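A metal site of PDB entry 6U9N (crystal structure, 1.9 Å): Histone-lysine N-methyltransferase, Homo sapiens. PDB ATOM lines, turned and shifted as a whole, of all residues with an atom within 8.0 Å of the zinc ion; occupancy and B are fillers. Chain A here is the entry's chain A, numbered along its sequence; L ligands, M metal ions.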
ATOM      1  N   ILE A  27       3.431  21.214   8.905  1.00  0.00           N
ATOM      2  CA  ILE A  27       4.141  20.098   9.522  1.00  0.00           C
ATOM      3  C   ILE A  27       3.285  19.578  10.689  1.00  0.00           C
ATOM      4  O   ILE A  27       2.891  18.404  10.664  1.00  0.00           O
ATOM      5  CB  ILE A  27       5.596  20.459   9.950  1.00  0.00           C
ATOM      6  CG1 ILE A  27       6.486  20.761   8.716  1.00  0.00           C
ATOM      7  CG2 ILE A  27       6.212  19.332  10.795  1.00  0.00           C
ATOM      8  CD1 ILE A  27       7.852  21.505   9.045  1.00  0.00           C
ATOM      9  N   HIS A  96      10.074  19.761  14.362  1.00  0.00           N
ATOM     10  CA  HIS A  96      11.188  18.925  13.887  1.00  0.00           C
ATOM     11  C   HIS A  96      11.213  18.888  12.345  1.00  0.00           C
ATOM     12  O   HIS A  96      10.156  18.960  11.717  1.00  0.00           O
ATOM     13  CB  HIS A  96      11.035  17.471  14.389  1.00  0.00           C
ATOM     14  CG  HIS A  96      11.955  16.496  13.709  1.00  0.00           C
ATOM     15  ND1 HIS A  96      13.289  16.387  14.065  1.00  0.00           N
ATOM     16  CD2 HIS A  96      11.707  15.664  12.674  1.00  0.00           C
ATOM     17  CE1 HIS A  96      13.807  15.494  13.238  1.00  0.00           C
ATOM     18  NE2 HIS A  96      12.897  15.028  12.383  1.00  0.00           N
ATOM     19  N   SER A  97      12.426  18.713  11.749  1.00  0.00           N
ATOM     20  CA  SER A  97      12.632  18.466  10.316  1.00  0.00           C
ATOM     21  C   SER A  97      13.909  17.715  10.132  1.00  0.00           C
ATOM     22  O   SER A  97      14.881  17.976  10.834  1.00  0.00           O
ATOM     23  CB  SER A  97      12.664  19.747   9.491  1.00  0.00           C
ATOM     24  OG  SER A  97      12.996  19.492   8.133  1.00  0.00           O
ATOM     25  N   CYS A  98      13.912  16.797   9.147  1.00  0.00           N
ATOM     26  CA  CYS A  98      15.016  15.931   8.775  1.00  0.00           C
ATOM     27  C   CYS A  98      16.003  16.652   7.856  1.00  0.00           C
ATOM     28  O   CYS A  98      17.107  16.165   7.619  1.00  0.00           O
ATOM     29  CB  CYS A  98      14.505  14.641   8.163  1.00  0.00           C
ATOM     30  SG  CYS A  98      13.288  13.787   9.199  1.00  0.00           S
ATOM     31  N   GLU A  99      15.586  17.820   7.339  1.00  0.00           N
ATOM     32  CA  GLU A  99      16.438  18.713   6.563  1.00  0.00           C
ATOM     33  C   GLU A  99      16.204  20.072   7.231  1.00  0.00           C
ATOM     34  O   GLU A  99      15.524  20.938   6.656  1.00  0.00           O
ATOM     35  CB  GLU A  99      16.072  18.703   5.067  1.00  0.00           C
ATOM     36  N   PRO A 145       5.492   9.386  13.648  1.00  0.00           N
ATOM     37  CA  PRO A 145       5.738   9.677  12.217  1.00  0.00           C
ATOM     38  C   PRO A 145       6.113  11.135  11.961  1.00  0.00           C
ATOM     39  O   PRO A 145       5.611  12.030  12.639  1.00  0.00           O
ATOM     40  CB  PRO A 145       4.414   9.303  11.530  1.00  0.00           C
ATOM     41  CG  PRO A 145       3.396   9.286  12.613  1.00  0.00           C
ATOM     42  CD  PRO A 145       4.104   8.939  13.879  1.00  0.00           C
ATOM     43  N   CYS A 146       7.058  11.371  11.031  1.00  0.00           N
ATOM     44  CA  CYS A 146       7.535  12.717  10.718  1.00  0.00           C
ATOM     45  C   CYS A 146       6.846  13.323   9.495  1.00  0.00           C
ATOM     46  O   CYS A 146       6.702  12.651   8.469  1.00  0.00           O
ATOM     47  CB  CYS A 146       9.048  12.725  10.543  1.00  0.00           C
ATOM     48  SG  CYS A 146       9.703  14.309  10.025  1.00  0.00           S
ATOM     49  N   ASN A 147       6.499  14.616   9.588  1.00  0.00           N
ATOM     50  CA  ASN A 147       5.804  15.380   8.547  1.00  0.00           C
ATOM     51  C   ASN A 147       6.611  16.541   7.972  1.00  0.00           C
ATOM     52  O   ASN A 147       6.039  17.437   7.356  1.00  0.00           O
ATOM     53  CB  ASN A 147       4.439  15.849   9.050  1.00  0.00           C
ATOM     54  CG  ASN A 147       3.435  16.114   7.959  1.00  0.00           C
ATOM     55  OD1 ASN A 147       3.204  15.294   7.060  1.00  0.00           O
ATOM     56  ND2 ASN A 147       2.817  17.280   8.007  1.00  0.00           N
ATOM     57  N   CYS A 148       7.952  16.525   8.118  1.00  0.00           N
ATOM     58  CA  CYS A 148       8.731  17.629   7.551  1.00  0.00           C
ATOM     59  C   CYS A 148       8.588  17.734   6.029  1.00  0.00           C
ATOM     60  O   CYS A 148       8.657  18.839   5.503  1.00  0.00           O
ATOM     61  CB  CYS A 148      10.196  17.563   7.981  1.00  0.00           C
ATOM     62  SG  CYS A 148      11.155  16.250   7.199  1.00  0.00           S
ATOM     63  N   GLY A 149       8.390  16.580   5.377  1.00  0.00           N
ATOM     64  CA  GLY A 149       8.181  16.454   3.929  1.00  0.00           C
ATOM     65  C   GLY A 149       9.436  16.533   3.097  1.00  0.00           C
ATOM     66  O   GLY A 149       9.350  16.644   1.873  1.00  0.00           O
ATOM     67  N   ALA A 150      10.628  16.478   3.739  1.00  0.00           N
ATOM     68  CA  ALA A 150      11.927  16.561   3.057  1.00  0.00           C
ATOM     69  C   ALA A 150      12.172  15.359   2.150  1.00  0.00           C
ATOM     70  O   ALA A 150      11.577  14.300   2.363  1.00  0.00           O
ATOM     71  CB  ALA A 150      13.046  16.712   4.072  1.00  0.00           C
ATOM     72  N   LYS A 151      13.029  15.511   1.135  1.00  0.00           N
ATOM     73  CA  LYS A 151      13.350  14.384   0.235  1.00  0.00           C
ATOM     74  C   LYS A 151      14.015  13.259   1.044  1.00  0.00           C
ATOM     75  O   LYS A 151      13.627  12.092   0.928  1.00  0.00           O
ATOM     76  CB  LYS A 151      14.266  14.846  -0.911  1.00  0.00           C
ATOM     77  N   LYS A 152      14.985  13.638   1.895  1.00  0.00           N
ATOM     78  CA  LYS A 152      15.770  12.740   2.735  1.00  0.00           C
ATOM     79  C   LYS A 152      15.168  12.577   4.150  1.00  0.00           C
ATOM     80  O   LYS A 152      15.890  12.555   5.146  1.00  0.00           O
ATOM     81  CB  LYS A 152      17.251  13.218   2.776  1.00  0.00           C
ATOM     82  CG  LYS A 152      18.001  13.163   1.426  1.00  0.00           C
ATOM     83  CD  LYS A 152      18.204  11.744   0.902  1.00  0.00           C
ATOM     84  CE  LYS A 152      19.268  11.647  -0.181  1.00  0.00           C
ATOM     85  NZ  LYS A 152      18.859  12.335  -1.442  1.00  0.00           N
ATOM     86  N   CYS A 153      13.827  12.456   4.224  1.00  0.00           N
ATOM     87  CA  CYS A 153      13.094  12.290   5.478  1.00  0.00           C
ATOM     88  C   CYS A 153      13.390  10.949   6.134  1.00  0.00           C
ATOM     89  O   CYS A 153      13.376   9.929   5.459  1.00  0.00           O
ATOM     90  CB  CYS A 153      11.599  12.495   5.264  1.00  0.00           C
ATOM     91  SG  CYS A 153      10.630  12.479   6.801  1.00  0.00           S
ATOM     92  N   ARG A 154      13.622  10.947   7.468  1.00  0.00           N
ATOM     93  CA  ARG A 154      13.870   9.745   8.283  1.00  0.00           C
ATOM     94  C   ARG A 154      12.522   9.053   8.592  1.00  0.00           C
ATOM     95  O   ARG A 154      12.499   7.953   9.160  1.00  0.00           O
ATOM     96  CB  ARG A 154      14.600  10.102   9.598  1.00  0.00           C
ATOM     97  CG  ARG A 154      15.905  10.893   9.429  1.00  0.00           C
ATOM     98  CD  ARG A 154      16.753  10.927  10.684  1.00  0.00           C
ATOM     99  NE  ARG A 154      16.279  11.917  11.664  1.00  0.00           N
ATOM    100  CZ  ARG A 154      15.515  11.626  12.712  1.00  0.00           C
ATOM    101  NH1 ARG A 154      15.143  12.576  13.558  1.00  0.00           N
ATOM    102  NH2 ARG A 154      15.108  10.377  12.929  1.00  0.00           N
ATOM    103  N   LYS A 155      11.398   9.721   8.245  1.00  0.00           N
ATOM    104  CA  LYS A 155      10.006   9.305   8.387  1.00  0.00           C
ATOM    105  C   LYS A 155       9.535   9.137   9.842  1.00  0.00           C
ATOM    106  O   LYS A 155       8.321   8.938  10.069  1.00  0.00           O
ATOM    107  CB  LYS A 155       9.699   8.064   7.535  1.00  0.00           C
ATOM    108  CG  LYS A 155      10.127   8.215   6.043  1.00  0.00           C
ATOM    109  CD  LYS A 155       9.197   9.115   5.220  1.00  0.00           C
ATOM    110  CE  LYS A 155       9.627   9.198   3.777  1.00  0.00           C
ATOM    111  NZ  LYS A 155       8.704  10.033   2.969  1.00  0.00           N
ATOM    112  N   PHE A 156      10.452   9.266  10.837  1.00  0.00           N
ATOM    113  CA  PHE A 156      10.140   9.216  12.288  1.00  0.00           C
ATOM    114  C   PHE A 156      10.958  10.226  13.091  1.00  0.00           C
ATOM    115  O   PHE A 156      12.122  10.479  12.758  1.00  0.00           O
ATOM    116  CB  PHE A 156      10.281   7.786  12.866  1.00  0.00           C
ATOM    117  CG  PHE A 156       9.399   6.756  12.198  1.00  0.00           C
ATOM    118  CD1 PHE A 156       8.085   6.560  12.619  1.00  0.00           C
ATOM    119  CD2 PHE A 156       9.871   5.994  11.122  1.00  0.00           C
ATOM    120  CE1 PHE A 156       7.256   5.629  11.974  1.00  0.00           C
ATOM    121  CE2 PHE A 156       9.038   5.074  10.472  1.00  0.00           C
ATOM    122  CZ  PHE A 156       7.745   4.902  10.910  1.00  0.00           C
ATOM    123  N   LEU A 157      10.336  10.822  14.129  1.00  0.00           N
ATOM    124  CA  LEU A 157      10.978  11.783  15.008  1.00  0.00           C
ATOM    125  C   LEU A 157      11.552  11.089  16.244  1.00  0.00           C
ATOM    126  O   LEU A 157      11.688   9.866  16.262  1.00  0.00           O
ATOM    127  CB  LEU A 157       9.983  12.886  15.426  1.00  0.00           C
HETATM  128  O1  LIG L   1       2.307  22.984  19.953  1.00  0.00           O
HETATM  129  C1  LIG L   1       2.532  22.863  18.754  1.00  0.00           C
HETATM  130  O2  LIG L   1       1.718  23.433  17.857  1.00  0.00           O
HETATM  131  C2  LIG L   1       3.679  22.111  18.095  1.00  0.00           C
HETATM  132  N1  LIG L   1       3.635  22.104  16.622  1.00  0.00           N
HETATM  133  C3  LIG L   1       4.993  22.759  18.564  1.00  0.00           C
HETATM  134  C4  LIG L   1       6.055  21.661  18.822  1.00  0.00           C
HETATM  135  N2  LIG L   1       5.660  20.577  19.782  1.00  0.00           N
HETATM  136  C5  LIG L   1       6.468  19.297  19.689  1.00  0.00           C
HETATM  137  C6  LIG L   1       5.528  18.256  19.063  1.00  0.00           C
HETATM  138  C7  LIG L   1       6.248  16.890  18.912  1.00  0.00           C
HETATM  139  O3  LIG L   1       6.206  16.124  20.080  1.00  0.00           O
HETATM  140  C8  LIG L   1       5.338  16.251  17.846  1.00  0.00           C
HETATM  141  O4  LIG L   1       4.157  15.824  18.389  1.00  0.00           O
HETATM  142  O5  LIG L   1       5.127  18.647  17.761  1.00  0.00           O
HETATM  143  C9  LIG L   1       4.965  17.520  16.963  1.00  0.00           C
HETATM  144  N3  LIG L   1       5.842  17.634  15.779  1.00  0.00           N
HETATM  145  C10 LIG L   1       5.798  16.891  14.608  1.00  0.00           C
HETATM  146  N4  LIG L   1       4.896  15.944  14.183  1.00  0.00           N
HETATM  147  C11 LIG L   1       5.230  15.422  12.995  1.00  0.00           C
HETATM  148  N5  LIG L   1       6.309  15.705  12.197  1.00  0.00           N
HETATM  149  C12 LIG L   1       6.981  18.480  15.668  1.00  0.00           C
HETATM  150  N6  LIG L   1       7.649  18.316  14.542  1.00  0.00           N
HETATM  151  C13 LIG L   1       6.940  17.308  13.866  1.00  0.00           C
HETATM  152  C14 LIG L   1       7.182  16.648  12.635  1.00  0.00           C
HETATM  153  N7  LIG L   1       8.265  16.947  11.867  1.00  0.00           N
HETATM  154  C15 LIG L   1       5.246  20.973  21.157  1.00  0.00           C
HETATM  155  C16 LIG L   1       4.312  19.908  21.795  1.00  0.00           C
HETATM  156  C17 LIG L   1       3.412  20.379  22.973  1.00  0.00           C
HETATM  157  N8  LIG L   1       2.305  20.679  21.973  1.00  0.00           N
HETATM  158  C18 LIG L   1       2.943  19.661  21.079  1.00  0.00           C
HETATM  159  C19 LIG L   1       0.919  20.378  22.476  1.00  0.00           C
HETATM  160  C20 LIG L   1      -0.001  20.177  21.295  1.00  0.00           C
HETATM  161  C21 LIG L   1      -0.352  21.278  20.492  1.00  0.00           C
HETATM  162  C22 LIG L   1      -1.153  21.087  19.339  1.00  0.00           C
HETATM  163  C23 LIG L   1      -1.595  19.790  19.024  1.00  0.00           C
HETATM  164 CL1  LIG L   1      -2.536  19.552  17.555  1.00  0.00          CL
HETATM  165  C24 LIG L   1      -1.283  18.678  19.820  1.00  0.00           C
HETATM  166  C25 LIG L   1      -0.473  18.878  20.966  1.00  0.00           C
HETATM  167 ZN    ZN M   1      11.284  14.297   8.345  1.00  0.00          ZN
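O of His 96 lies within hydrogen-bond range of N7 of the ligand (2.8 Å). The backbone NH (N) of Asn 147 is in hydrogen-bond range of a nitrogen (N5) of the ligand (2.8 Å). A nitrogen (N7) of the ligand sits close to the side-chain sulfur of Cys 146 (3.5 Å). N of His 96 sits at hydrogen-bond distance from N6 of the ligand, at 2.8 Å.
Along chain A the residues within 4 Å of the zinc ion span positions 98 to 153.
The side-chain sulfur (SG) of Cys 148 lies close to the backbone NH (N) of Ala 150 (3.5 Å). The side-chain sulfur (SG) of Cys 98 lies close to a ring nitrogen (NE2) of His 96, at 3.4 Å. The side-chain sulfur of Cys 98 lies close to the backbone NH of Arg 154 (3.3 Å). N of Cys 146 sits at hydrogen-bond distance from O of Lys 155 (2.9 Å). The side-chain sulfur of Cys 153 sits close to the backbone NH of Lys 155, at 3.2 Å.
The zinc ion is bound by SG of Cys 98 (2.2 Å), SG of Cys 148 (2.3 Å), SG of Cys 146 (2.3 Å) and SG of Cys 153 (2.5 Å).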
